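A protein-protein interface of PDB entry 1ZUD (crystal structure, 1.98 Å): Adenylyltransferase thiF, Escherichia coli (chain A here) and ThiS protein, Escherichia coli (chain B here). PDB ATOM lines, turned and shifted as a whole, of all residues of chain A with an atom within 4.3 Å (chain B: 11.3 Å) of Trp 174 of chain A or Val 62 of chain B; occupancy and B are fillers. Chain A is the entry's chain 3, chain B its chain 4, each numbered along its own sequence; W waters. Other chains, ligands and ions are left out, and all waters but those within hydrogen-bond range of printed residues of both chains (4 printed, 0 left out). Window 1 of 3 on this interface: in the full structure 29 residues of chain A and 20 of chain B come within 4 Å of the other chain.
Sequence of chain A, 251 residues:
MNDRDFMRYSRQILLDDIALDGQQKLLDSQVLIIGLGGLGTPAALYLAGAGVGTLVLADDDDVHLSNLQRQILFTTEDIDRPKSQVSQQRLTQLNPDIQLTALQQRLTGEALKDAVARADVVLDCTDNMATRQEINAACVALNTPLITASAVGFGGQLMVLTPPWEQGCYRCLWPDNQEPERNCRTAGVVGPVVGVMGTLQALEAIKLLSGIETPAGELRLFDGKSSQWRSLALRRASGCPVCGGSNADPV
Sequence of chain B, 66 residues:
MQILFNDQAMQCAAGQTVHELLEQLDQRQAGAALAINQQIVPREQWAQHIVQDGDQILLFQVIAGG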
ATOM      1  N   MET A 129      -9.967 -17.456   5.483  1.00  0.00           N
ATOM      2  CA  MET A 129      -9.474 -18.668   6.117  1.00  0.00           C
ATOM      3  C   MET A 129     -10.425 -19.287   7.119  1.00  0.00           C
ATOM      4  O   MET A 129     -10.647 -20.477   7.089  1.00  0.00           O
ATOM      5  CB  MET A 129      -8.167 -18.395   6.875  1.00  0.00           C
ATOM      6  CG  MET A 129      -7.087 -17.742   6.072  1.00  0.00           C
ATOM      7  SD  MET A 129      -5.949 -19.019   5.640  1.00  0.00           S
ATOM      8  CE  MET A 129      -6.751 -19.507   4.221  1.00  0.00           C
ATOM      9  N   GLN A 133     -11.770 -22.981   6.887  1.00  0.00           N
ATOM     10  CA  GLN A 133     -11.470 -24.064   7.846  1.00  0.00           C
ATOM     11  C   GLN A 133     -12.760 -24.715   8.368  1.00  0.00           C
ATOM     12  O   GLN A 133     -12.823 -25.954   8.526  1.00  0.00           O
ATOM     13  CB  GLN A 133     -10.648 -23.530   9.035  1.00  0.00           C
ATOM     14  CG  GLN A 133      -9.298 -23.014   8.624  1.00  0.00           C
ATOM     15  CD  GLN A 133      -8.307 -24.140   8.348  1.00  0.00           C
ATOM     16  OE1 GLN A 133      -8.673 -25.318   8.360  1.00  0.00           O
ATOM     17  NE2 GLN A 133      -7.048 -23.775   8.082  1.00  0.00           N
ATOM     18  N   GLN A 157      -5.228 -21.188  -6.737  1.00  0.00           N
ATOM     19  CA  GLN A 157      -4.927 -22.448  -6.059  1.00  0.00           C
ATOM     20  C   GLN A 157      -6.173 -23.298  -6.113  1.00  0.00           C
ATOM     21  O   GLN A 157      -7.260 -22.790  -5.918  1.00  0.00           O
ATOM     22  CB  GLN A 157      -4.532 -22.196  -4.576  1.00  0.00           C
ATOM     23  CG  GLN A 157      -3.328 -21.231  -4.471  1.00  0.00           C
ATOM     24  CD  GLN A 157      -2.823 -20.969  -3.017  1.00  0.00           C
ATOM     25  OE1 GLN A 157      -3.566 -21.143  -2.062  1.00  0.00           O
ATOM     26  NE2 GLN A 157      -1.573 -20.511  -2.887  1.00  0.00           N
ATOM     27  N   TYR A 170      -7.892 -29.865   4.154  1.00  0.00           N
ATOM     28  CA  TYR A 170      -7.410 -28.469   3.952  1.00  0.00           C
ATOM     29  C   TYR A 170      -6.531 -28.036   5.131  1.00  0.00           C
ATOM     30  O   TYR A 170      -5.529 -27.307   4.977  1.00  0.00           O
ATOM     31  CB  TYR A 170      -8.602 -27.507   3.844  1.00  0.00           C
ATOM     32  CG  TYR A 170      -8.249 -26.051   3.535  1.00  0.00           C
ATOM     33  CD1 TYR A 170      -8.123 -25.600   2.217  1.00  0.00           C
ATOM     34  CD2 TYR A 170      -8.138 -25.123   4.562  1.00  0.00           C
ATOM     35  CE1 TYR A 170      -7.909 -24.227   1.931  1.00  0.00           C
ATOM     36  CE2 TYR A 170      -7.930 -23.794   4.299  1.00  0.00           C
ATOM     37  CZ  TYR A 170      -7.821 -23.348   2.986  1.00  0.00           C
ATOM     38  OH  TYR A 170      -7.643 -22.007   2.794  1.00  0.00           O
ATOM     39  N   ARG A 171      -6.915 -28.511   6.313  1.00  0.00           N
ATOM     40  CA  ARG A 171      -6.185 -28.208   7.542  1.00  0.00           C
ATOM     41  C   ARG A 171      -4.820 -28.920   7.601  1.00  0.00           C
ATOM     42  O   ARG A 171      -3.941 -28.459   8.318  1.00  0.00           O
ATOM     43  CB  ARG A 171      -7.054 -28.562   8.771  1.00  0.00           C
ATOM     44  CG  ARG A 171      -6.338 -28.539  10.135  1.00  0.00           C
ATOM     45  CD  ARG A 171      -6.106 -27.159  10.670  1.00  0.00           C
ATOM     46  NE  ARG A 171      -5.375 -27.188  11.946  1.00  0.00           N
ATOM     47  CZ  ARG A 171      -4.113 -27.603  12.096  1.00  0.00           C
ATOM     48  NH1 ARG A 171      -3.379 -28.056  11.065  1.00  0.00           N
ATOM     49  NH2 ARG A 171      -3.556 -27.538  13.292  1.00  0.00           N
ATOM     50  N   CYS A 172      -4.603 -29.989   6.849  1.00  0.00           N
ATOM     51  CA  CYS A 172      -3.250 -30.617   6.855  1.00  0.00           C
ATOM     52  C   CYS A 172      -2.250 -29.703   6.153  1.00  0.00           C
ATOM     53  O   CYS A 172      -1.062 -29.654   6.486  1.00  0.00           O
ATOM     54  CB  CYS A 172      -3.204 -31.969   6.118  1.00  0.00           C
ATOM     55  SG  CYS A 172      -4.146 -33.328   6.893  1.00  0.00           S
ATOM     56  N   LEU A 173      -2.737 -28.979   5.151  1.00  0.00           N
ATOM     57  CA  LEU A 173      -1.892 -28.079   4.371  1.00  0.00           C
ATOM     58  C   LEU A 173      -1.733 -26.699   5.005  1.00  0.00           C
ATOM     59  O   LEU A 173      -0.653 -26.116   4.982  1.00  0.00           O
ATOM     60  CB  LEU A 173      -2.520 -27.923   2.961  1.00  0.00           C
ATOM     61  CG  LEU A 173      -1.880 -26.928   1.995  1.00  0.00           C
ATOM     62  CD1 LEU A 173      -0.417 -27.350   1.764  1.00  0.00           C
ATOM     63  CD2 LEU A 173      -2.667 -26.934   0.628  1.00  0.00           C
ATOM     64  N   TRP A 174      -2.855 -26.147   5.478  1.00  0.00           N
ATOM     65  CA  TRP A 174      -2.921 -24.832   6.085  1.00  0.00           C
ATOM     66  C   TRP A 174      -3.365 -24.929   7.545  1.00  0.00           C
ATOM     67  O   TRP A 174      -4.571 -25.111   7.860  1.00  0.00           O
ATOM     68  CB  TRP A 174      -3.949 -23.937   5.332  1.00  0.00           C
ATOM     69  CG  TRP A 174      -3.632 -23.781   3.850  1.00  0.00           C
ATOM     70  CD1 TRP A 174      -4.436 -24.146   2.805  1.00  0.00           C
ATOM     71  CD2 TRP A 174      -2.428 -23.248   3.264  1.00  0.00           C
ATOM     72  NE1 TRP A 174      -3.807 -23.874   1.612  1.00  0.00           N
ATOM     73  CE2 TRP A 174      -2.579 -23.322   1.858  1.00  0.00           C
ATOM     74  CE3 TRP A 174      -1.239 -22.703   3.792  1.00  0.00           C
ATOM     75  CZ2 TRP A 174      -1.592 -22.884   0.965  1.00  0.00           C
ATOM     76  CZ3 TRP A 174      -0.251 -22.257   2.907  1.00  0.00           C
ATOM     77  CH2 TRP A 174      -0.435 -22.352   1.509  1.00  0.00           C
ATOM     78  N   PRO A 175      -2.404 -24.806   8.464  1.00  0.00           N
ATOM     79  CA  PRO A 175      -2.804 -24.883   9.874  1.00  0.00           C
ATOM     80  C   PRO A 175      -3.403 -23.532  10.288  1.00  0.00           C
ATOM     81  O   PRO A 175      -4.139 -23.445  11.251  1.00  0.00           O
ATOM     82  CB  PRO A 175      -1.479 -25.164  10.618  1.00  0.00           C
ATOM     83  CG  PRO A 175      -0.560 -25.795   9.560  1.00  0.00           C
ATOM     84  CD  PRO A 175      -0.953 -25.034   8.276  1.00  0.00           C
ATOM     85  N   ASP A 176      -3.120 -22.482   9.520  1.00  0.00           N
ATOM     86  CA  ASP A 176      -3.576 -21.115   9.857  1.00  0.00           C
ATOM     87  C   ASP A 176      -5.076 -20.878   9.835  1.00  0.00           C
ATOM     88  O   ASP A 176      -5.789 -21.383   8.952  1.00  0.00           O
ATOM     89  CB  ASP A 176      -2.945 -20.089   8.897  1.00  0.00           C
ATOM     90  CG  ASP A 176      -1.535 -20.466   8.478  1.00  0.00           C
ATOM     91  OD1 ASP A 176      -0.564 -19.942   9.062  1.00  0.00           O
ATOM     92  OD2 ASP A 176      -1.410 -21.310   7.563  1.00  0.00           O
ATOM     93  N   GLU A 179      -5.076 -15.102   7.482  1.00  0.00           N
ATOM     94  CA  GLU A 179      -3.894 -14.865   6.636  1.00  0.00           C
ATOM     95  C   GLU A 179      -2.849 -14.147   7.499  1.00  0.00           C
ATOM     96  O   GLU A 179      -3.180 -13.585   8.548  1.00  0.00           O
ATOM     97  CB  GLU A 179      -4.235 -14.038   5.402  1.00  0.00           C
ATOM     98  CG  GLU A 179      -4.627 -14.900   4.194  1.00  0.00           C
ATOM     99  CD  GLU A 179      -5.454 -14.130   3.157  1.00  0.00           C
ATOM    100  OE1 GLU A 179      -5.289 -14.361   1.930  1.00  0.00           O
ATOM    101  OE2 GLU A 179      -6.287 -13.299   3.582  1.00  0.00           O
ATOM    102  N   LEU B  22      14.796 -22.031   6.407  1.00  0.00           N
ATOM    103  CA  LEU B  22      13.868 -20.890   6.282  1.00  0.00           C
ATOM    104  C   LEU B  22      14.365 -19.742   7.172  1.00  0.00           C
ATOM    105  O   LEU B  22      14.265 -18.562   6.812  1.00  0.00           O
ATOM    106  CB  LEU B  22      12.419 -21.314   6.650  1.00  0.00           C
ATOM    107  CG  LEU B  22      11.839 -22.406   5.711  1.00  0.00           C
ATOM    108  CD1 LEU B  22      10.402 -22.729   6.096  1.00  0.00           C
ATOM    109  CD2 LEU B  22      11.904 -21.921   4.244  1.00  0.00           C
ATOM    110  N   GLN B  27      12.688 -16.260   6.083  1.00  0.00           N
ATOM    111  CA  GLN B  27      11.312 -16.455   5.599  1.00  0.00           C
ATOM    112  C   GLN B  27      10.344 -16.712   6.750  1.00  0.00           C
ATOM    113  O   GLN B  27      10.655 -17.456   7.702  1.00  0.00           O
ATOM    114  CB  GLN B  27      11.255 -17.648   4.649  1.00  0.00           C
ATOM    115  CG  GLN B  27      11.964 -17.427   3.331  1.00  0.00           C
ATOM    116  CD  GLN B  27      11.399 -16.200   2.603  1.00  0.00           C
ATOM    117  OE1 GLN B  27      10.182 -16.063   2.434  1.00  0.00           O
ATOM    118  NE2 GLN B  27      12.283 -15.300   2.196  1.00  0.00           N
ATOM    119  N   ARG B  28       9.163 -16.105   6.648  1.00  0.00           N
ATOM    120  CA  ARG B  28       8.110 -16.275   7.648  1.00  0.00           C
ATOM    121  C   ARG B  28       7.389 -17.617   7.398  1.00  0.00           C
ATOM    122  O   ARG B  28       7.088 -17.959   6.253  1.00  0.00           O
ATOM    123  CB  ARG B  28       7.122 -15.094   7.544  1.00  0.00           C
ATOM    124  CG  ARG B  28       5.717 -15.411   7.988  1.00  0.00           C
ATOM    125  CD  ARG B  28       4.719 -14.832   6.989  1.00  0.00           C
ATOM    126  NE  ARG B  28       4.322 -13.469   7.316  1.00  0.00           N
ATOM    127  CZ  ARG B  28       3.875 -12.580   6.429  1.00  0.00           C
ATOM    128  NH1 ARG B  28       3.778 -12.901   5.144  1.00  0.00           N
ATOM    129  NH2 ARG B  28       3.488 -11.378   6.839  1.00  0.00           N
ATOM    130  N   GLN B  29       7.080 -18.351   8.463  1.00  0.00           N
ATOM    131  CA  GLN B  29       6.432 -19.653   8.316  1.00  0.00           C
ATOM    132  C   GLN B  29       4.889 -19.634   8.332  1.00  0.00           C
ATOM    133  O   GLN B  29       4.238 -20.468   7.704  1.00  0.00           O
ATOM    134  CB  GLN B  29       7.004 -20.598   9.385  1.00  0.00           C
ATOM    135  CG  GLN B  29       8.516 -20.792   9.169  1.00  0.00           C
ATOM    136  CD  GLN B  29       9.142 -21.758  10.176  1.00  0.00           C
ATOM    137  OE1 GLN B  29       8.469 -22.662  10.704  1.00  0.00           O
ATOM    138  NE2 GLN B  29      10.436 -21.570  10.444  1.00  0.00           N
ATOM    139  N   ALA B  30       4.335 -18.666   9.051  1.00  0.00           N
ATOM    140  CA  ALA B  30       2.903 -18.481   9.169  1.00  0.00           C
ATOM    141  C   ALA B  30       2.329 -18.192   7.761  1.00  0.00           C
ATOM    142  O   ALA B  30       2.869 -17.390   7.013  1.00  0.00           O
ATOM    143  CB  ALA B  30       2.616 -17.315  10.121  1.00  0.00           C
ATOM    144  N   GLY B  31       1.258 -18.879   7.399  1.00  0.00           N
ATOM    145  CA  GLY B  31       0.668 -18.658   6.091  1.00  0.00           C
ATOM    146  C   GLY B  31       1.456 -19.255   4.933  1.00  0.00           C
ATOM    147  O   GLY B  31       1.101 -19.014   3.783  1.00  0.00           O
ATOM    148  N   ALA B  32       2.504 -20.048   5.207  1.00  0.00           N
ATOM    149  CA  ALA B  32       3.299 -20.635   4.122  1.00  0.00           C
ATOM    150  C   ALA B  32       3.206 -22.142   4.039  1.00  0.00           C
ATOM    151  O   ALA B  32       2.898 -22.809   5.019  1.00  0.00           O
ATOM    152  CB  ALA B  32       4.817 -20.208   4.277  1.00  0.00           C
ATOM    153  N   ALA B  33       3.410 -22.700   2.853  1.00  0.00           N
ATOM    154  CA  ALA B  33       3.414 -24.154   2.756  1.00  0.00           C
ATOM    155  C   ALA B  33       4.672 -24.403   1.949  1.00  0.00           C
ATOM    156  O   ALA B  33       5.165 -23.514   1.260  1.00  0.00           O
ATOM    157  CB  ALA B  33       2.154 -24.707   2.027  1.00  0.00           C
ATOM    158  N   LEU B  34       5.191 -25.610   2.042  1.00  0.00           N
ATOM    159  CA  LEU B  34       6.434 -25.944   1.374  1.00  0.00           C
ATOM    160  C   LEU B  34       6.342 -27.312   0.655  1.00  0.00           C
ATOM    161  O   LEU B  34       5.722 -28.268   1.157  1.00  0.00           O
ATOM    162  CB  LEU B  34       7.568 -25.936   2.445  1.00  0.00           C
ATOM    163  CG  LEU B  34       8.959 -26.221   1.870  1.00  0.00           C
ATOM    164  CD1 LEU B  34       9.865 -25.046   2.181  1.00  0.00           C
ATOM    165  CD2 LEU B  34       9.502 -27.540   2.387  1.00  0.00           C
ATOM    166  N   ALA B  35       6.926 -27.390  -0.539  1.00  0.00           N
ATOM    167  CA  ALA B  35       6.967 -28.644  -1.260  1.00  0.00           C
ATOM    168  C   ALA B  35       8.435 -28.981  -1.519  1.00  0.00           C
ATOM    169  O   ALA B  35       9.270 -28.075  -1.720  1.00  0.00           O
ATOM    170  CB  ALA B  35       6.257 -28.534  -2.577  1.00  0.00           C
ATOM    171  N   ILE B  40       4.173 -31.903  -0.921  1.00  0.00           N
ATOM    172  CA  ILE B  40       4.061 -31.034   0.234  1.00  0.00           C
ATOM    173  C   ILE B  40       4.718 -31.716   1.445  1.00  0.00           C
ATOM    174  O   ILE B  40       4.577 -32.913   1.624  1.00  0.00           O
ATOM    175  CB  ILE B  40       2.589 -30.823   0.615  1.00  0.00           C
ATOM    176  CG1 ILE B  40       1.866 -30.132  -0.571  1.00  0.00           C
ATOM    177  CG2 ILE B  40       2.495 -29.991   1.932  1.00  0.00           C
ATOM    178  CD1 ILE B  40       2.327 -28.696  -0.790  1.00  0.00           C
ATOM    179  N   VAL B  41       5.399 -30.919   2.248  1.00  0.00           N
ATOM    180  CA  VAL B  41       6.011 -31.353   3.491  1.00  0.00           C
ATOM    181  C   VAL B  41       5.207 -30.577   4.557  1.00  0.00           C
ATOM    182  O   VAL B  41       5.355 -29.370   4.683  1.00  0.00           O
ATOM    183  CB  VAL B  41       7.496 -30.954   3.613  1.00  0.00           C
ATOM    184  CG1 VAL B  41       8.004 -31.435   4.993  1.00  0.00           C
ATOM    185  CG2 VAL B  41       8.325 -31.624   2.525  1.00  0.00           C
ATOM    186  N   PRO B  42       4.324 -31.259   5.297  1.00  0.00           N
ATOM    187  CA  PRO B  42       3.518 -30.595   6.326  1.00  0.00           C
ATOM    188  C   PRO B  42       4.399 -29.776   7.282  1.00  0.00           C
ATOM    189  O   PRO B  42       5.446 -30.222   7.724  1.00  0.00           O
ATOM    190  CB  PRO B  42       2.797 -31.759   7.008  1.00  0.00           C
ATOM    191  CG  PRO B  42       2.673 -32.786   5.941  1.00  0.00           C
ATOM    192  CD  PRO B  42       4.051 -32.727   5.278  1.00  0.00           C
ATOM    193  N   ARG B  43       3.943 -28.576   7.607  1.00  0.00           N
ATOM    194  CA  ARG B  43       4.685 -27.665   8.454  1.00  0.00           C
ATOM    195  C   ARG B  43       5.088 -28.298   9.772  1.00  0.00           C
ATOM    196  O   ARG B  43       6.123 -27.958  10.329  1.00  0.00           O
ATOM    197  CB  ARG B  43       3.840 -26.434   8.752  1.00  0.00           C
ATOM    198  CG  ARG B  43       4.631 -25.190   8.928  1.00  0.00           C
ATOM    199  CD  ARG B  43       3.841 -24.070   8.264  1.00  0.00           C
ATOM    200  NE  ARG B  43       3.151 -23.318   9.276  1.00  0.00           N
ATOM    201  CZ  ARG B  43       2.087 -22.545   9.058  1.00  0.00           C
ATOM    202  NH1 ARG B  43       1.526 -22.381   7.814  1.00  0.00           N
ATOM    203  NH2 ARG B  43       1.582 -21.939  10.125  1.00  0.00           N
ATOM    204  N   GLU B  44       4.264 -29.217  10.265  1.00  0.00           N
ATOM    205  CA  GLU B  44       4.569 -29.836  11.538  1.00  0.00           C
ATOM    206  C   GLU B  44       5.864 -30.637  11.439  1.00  0.00           C
ATOM    207  O   GLU B  44       6.400 -31.038  12.447  1.00  0.00           O
ATOM    208  CB  GLU B  44       3.394 -30.720  12.006  1.00  0.00           C
ATOM    209  CG  GLU B  44       3.180 -32.005  11.212  1.00  0.00           C
ATOM    210  CD  GLU B  44       1.996 -32.841  11.735  1.00  0.00           C
ATOM    211  OE1 GLU B  44       1.841 -34.007  11.297  1.00  0.00           O
ATOM    212  OE2 GLU B  44       1.212 -32.331  12.577  1.00  0.00           O
ATOM    213  N   TRP B  46       8.689 -29.470   9.654  1.00  0.00           N
ATOM    214  CA  TRP B  46       9.834 -28.656   9.256  1.00  0.00           C
ATOM    215  C   TRP B  46      10.997 -28.600  10.228  1.00  0.00           C
ATOM    216  O   TRP B  46      12.120 -28.420   9.797  1.00  0.00           O
ATOM    217  CB  TRP B  46       9.440 -27.210   8.893  1.00  0.00           C
ATOM    218  CG  TRP B  46       8.427 -27.074   7.724  1.00  0.00           C
ATOM    219  CD1 TRP B  46       7.988 -28.053   6.879  1.00  0.00           C
ATOM    220  CD2 TRP B  46       7.768 -25.871   7.308  1.00  0.00           C
ATOM    221  NE1 TRP B  46       7.085 -27.539   5.958  1.00  0.00           N
ATOM    222  CE2 TRP B  46       6.934 -26.201   6.198  1.00  0.00           C
ATOM    223  CE3 TRP B  46       7.794 -24.559   7.757  1.00  0.00           C
ATOM    224  CZ2 TRP B  46       6.129 -25.250   5.541  1.00  0.00           C
ATOM    225  CZ3 TRP B  46       6.969 -23.592   7.081  1.00  0.00           C
ATOM    226  CH2 TRP B  46       6.163 -23.966   5.999  1.00  0.00           C
ATOM    227  N   LEU B  58       9.923 -25.377  -3.015  1.00  0.00           N
ATOM    228  CA  LEU B  58       8.994 -24.270  -3.306  1.00  0.00           C
ATOM    229  C   LEU B  58       8.420 -23.831  -1.974  1.00  0.00           C
ATOM    230  O   LEU B  58       7.973 -24.653  -1.159  1.00  0.00           O
ATOM    231  CB  LEU B  58       7.816 -24.742  -4.160  1.00  0.00           C
ATOM    232  CG  LEU B  58       8.126 -25.378  -5.499  1.00  0.00           C
ATOM    233  CD1 LEU B  58       6.813 -25.620  -6.226  1.00  0.00           C
ATOM    234  CD2 LEU B  58       9.042 -24.424  -6.325  1.00  0.00           C
ATOM    235  N   LEU B  59       8.455 -22.539  -1.747  1.00  0.00           N
ATOM    236  CA  LEU B  59       7.912 -21.968  -0.547  1.00  0.00           C
ATOM    237  C   LEU B  59       6.870 -20.963  -1.067  1.00  0.00           C
ATOM    238  O   LEU B  59       7.224 -20.065  -1.821  1.00  0.00           O
ATOM    239  CB  LEU B  59       9.007 -21.238   0.194  1.00  0.00           C
ATOM    240  CG  LEU B  59       8.412 -20.528   1.384  1.00  0.00           C
ATOM    241  CD1 LEU B  59       7.913 -21.592   2.390  1.00  0.00           C
ATOM    242  CD2 LEU B  59       9.465 -19.567   1.960  1.00  0.00           C
ATOM    243  N   PHE B  60       5.604 -21.116  -0.710  1.00  0.00           N
ATOM    244  CA  PHE B  60       4.572 -20.184  -1.238  1.00  0.00           C
ATOM    245  C   PHE B  60       3.529 -19.849  -0.171  1.00  0.00           C
ATOM    246  O   PHE B  60       3.392 -20.541   0.835  1.00  0.00           O
ATOM    247  CB  PHE B  60       3.880 -20.795  -2.497  1.00  0.00           C
ATOM    248  CG  PHE B  60       3.358 -22.220  -2.285  1.00  0.00           C
ATOM    249  CD1 PHE B  60       4.240 -23.314  -2.263  1.00  0.00           C
ATOM    250  CD2 PHE B  60       2.013 -22.450  -2.030  1.00  0.00           C
ATOM    251  CE1 PHE B  60       3.774 -24.620  -1.981  1.00  0.00           C
ATOM    252  CE2 PHE B  60       1.531 -23.742  -1.754  1.00  0.00           C
ATOM    253  CZ  PHE B  60       2.424 -24.843  -1.730  1.00  0.00           C
ATOM    254  N   GLN B  61       2.768 -18.792  -0.397  1.00  0.00           N
ATOM    255  CA  GLN B  61       1.777 -18.393   0.604  1.00  0.00           C
ATOM    256  C   GLN B  61       0.390 -18.834   0.226  1.00  0.00           C
ATOM    257  O   GLN B  61       0.093 -19.031  -0.969  1.00  0.00           O
ATOM    258  CB  GLN B  61       1.780 -16.869   0.752  1.00  0.00           C
ATOM    259  CG  GLN B  61       2.996 -16.343   1.480  1.00  0.00           C
ATOM    260  CD  GLN B  61       2.747 -16.211   2.980  1.00  0.00           C
ATOM    261  OE1 GLN B  61       1.717 -15.666   3.391  1.00  0.00           O
ATOM    262  NE2 GLN B  61       3.688 -16.697   3.802  1.00  0.00           N
ATOM    263  N   VAL B  62      -0.451 -18.996   1.246  1.00  0.00           N
ATOM    264  CA  VAL B  62      -1.825 -19.381   1.002  1.00  0.00           C
ATOM    265  C   VAL B  62      -2.593 -18.201   0.324  1.00  0.00           C
ATOM    266  O   VAL B  62      -2.325 -17.016   0.608  1.00  0.00           O
ATOM    267  CB  VAL B  62      -2.555 -19.727   2.338  1.00  0.00           C
ATOM    268  CG1 VAL B  62      -2.524 -18.474   3.341  1.00  0.00           C
ATOM    269  CG2 VAL B  62      -4.027 -20.229   2.014  1.00  0.00           C
ATOM    270  N   ILE B  63      -3.517 -18.525  -0.584  1.00  0.00           N
ATOM    271  CA  ILE B  63      -4.362 -17.468  -1.158  1.00  0.00           C
ATOM    272  C   ILE B  63      -5.728 -17.882  -0.600  1.00  0.00           C
ATOM    273  O   ILE B  63      -6.149 -19.024  -0.755  1.00  0.00           O
ATOM    274  CB  ILE B  63      -4.431 -17.517  -2.716  1.00  0.00           C
ATOM    275  CG1 ILE B  63      -3.061 -17.174  -3.311  1.00  0.00           C
ATOM    276  CG2 ILE B  63      -5.596 -16.598  -3.233  1.00  0.00           C
ATOM    277  CD1 ILE B  63      -2.911 -17.461  -4.810  1.00  0.00           C
ATOM    278  N   ALA B  64      -6.418 -16.953   0.033  1.00  0.00           N
ATOM    279  CA  ALA B  64      -7.730 -17.242   0.592  1.00  0.00           C
ATOM    280  C   ALA B  64      -8.872 -16.513  -0.139  1.00  0.00           C
ATOM    281  O   ALA B  64     -10.006 -16.864   0.054  1.00  0.00           O
ATOM    282  CB  ALA B  64      -7.746 -16.877   2.044  1.00  0.00           C
ATOM    283  N   GLY B  65      -8.569 -15.569  -1.020  1.00  0.00           N
ATOM    284  CA  GLY B  65      -9.640 -14.826  -1.728  1.00  0.00           C
ATOM    285  C   GLY B  65     -10.483 -15.605  -2.734  1.00  0.00           C
ATOM    286  O   GLY B  65     -10.119 -16.704  -3.100  1.00  0.00           O
ATOM    287  N   GLY B  66     -11.587 -15.038  -3.222  1.00  0.00           N
ATOM    288  CA  GLY B  66     -12.433 -15.788  -4.141  1.00  0.00           C
ATOM    289  C   GLY B  66     -13.527 -14.987  -4.831  1.00  0.00           C
ATOM    290  O   GLY B  66     -14.666 -15.495  -5.088  1.00  0.00           O
ATOM    291  OXT GLY B  66     -13.210 -13.831  -5.159  1.00  0.00           O
HETATM  292  O   HOH W   1      -7.295 -21.539   0.250  1.00  0.00           O
HETATM  293  O   HOH W   2      -5.793 -13.803  -0.470  1.00  0.00           O
HETATM  294  O   HOH W   3       1.126 -27.997   6.911  1.00  0.00           O
HETATM  295  O   HOH W   4       1.963 -25.627   5.322  1.00  0.00           O
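Of the 11 printed residues of chain A, 7 touch a printed residue of chain B. Hydrophobic or aromatic side chains of chain A within 4 Å of the printed part of chain B: Met 129, Leu 173, Trp 174 and Pro 175. Of the 25 printed residues of chain B, 10 touch a printed residue of chain A. Printed residues of chain B that touch a printed residue of chain A: Ala 30, Gly 31, Ala 32, Ala 33, Ile 40, Arg 43, Gln 61, Val 62, Ile 63 and Ala 64. Hydrophobic or aromatic side chains of chain B within 4 Å of the printed part of chain A: Ala 33, Ile 40, Val 62, Ile 63 and Ala 64.
Trp 174 of chain A touches just these residues of chain B: Gly 31 (3.6 Å), Ala 32 (3.6 Å), Ala 33 (3.5 Å), Gln 61 (3.8 Å) and Val 62 (3.3 Å). Of the printed residues of chain A, Val 62 of chain B touches Met 129 (3.6 Å), Gln 157 (3.9 Å) and Trp 174 (3.3 Å). Of chain B, only Arg 43 (3.7 Å) comes within 4 Å of Pro 175 of chain A. Asp 176 of chain A touches just these residues of chain B: Ala 30, Gly 31 and Arg 43. Glu 179 of chain A touches just one residue of chain B: Ala 64. Printed residues of chain A within 4 Å of Gln 61 of chain B: Gln 157 (2.9 Å) and Trp 174 (3.8 Å). Of the printed residues of chain A, Ile 63 of chain B touches Gln 157. Printed residues of chain A within 4 Å of Ile 40 of chain B: Leu 173. The nearest residue of chain A that does not touch Val 62 of chain B is Tyr 170 of chain A (4.1 Å).
The side-chain carboxylate (OD1) of Asp 176 of chain A is in hydrogen-bond range of the backbone NH (N) of Gly 31 of chain B, at 2.7 Å. The side-chain carboxylate of Asp 176 of chain A lies within salt-bridge range of the guanidinium group of Arg 43 of chain B (3.1 Å). The backbone NH (N) of Ile 63 of chain B is in hydrogen-bond range of the side-chain amide oxygen (OE1) of Gln 157 of chain A, at 3.0 Å. The side-chain amide nitrogen of Gln 157 of chain A sits at hydrogen-bond distance from the backbone carbonyl oxygen of Gln 61 of chain B, 2.9 Å away. OE1 of Glu 179 of chain A is in hydrogen-bond range of N of Ala 64 of chain B.
Among the printed residues, merely in contact across the chains: Met 129 of chain A with Val 62 of chain B, Met 129 of chain A with Ala 64 of chain B, Gln 157 of chain A with Val 62 of chain B, Leu 173 of chain A with Ala 33 of chain B, Leu 173 of chain A with Ile 40 of chain B, Trp 174 of chain A with Gly 31 of chain B, Trp 174 of chain A with Ala 32 of chain B, Trp 174 of chain A with Ala 33 of chain B, Trp 174 of chain A with Gln 61 of chain B, Trp 174 of chain A with Val 62 of chain B, Pro 175 of chain A with Arg 43 of chain B and Asp 176 of chain A with Ala 30 of chain B.
The backbone carbonyl oxygen (O) of Ala 30 of chain B lies within hydrogen-bond range of the side-chain amide nitrogen (NE2) of Gln 61 of chain B. The side-chain amide nitrogen (NE2) of Gln 133 of chain A is in hydrogen-bond range of the backbone carbonyl oxygen (O) of Trp 174 of chain A (2.8 Å).
Water W2 lies within hydrogen-bond range of OE1 of Glu 179 of chain A, N of Ala 64 of chain B and N of Gly 65 of chain B. Water W1 bridges OH of Tyr 170 of chain A (2.6 Å) and O of Ile 63 of chain B (2.9 Å). Water W3 lies within hydrogen-bond range of the backbone carbonyl oxygen of Cys 172 of chain A, the backbone NH of Arg 43 of chain B and the backbone carbonyl oxygen of Leu 173 of chain A.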
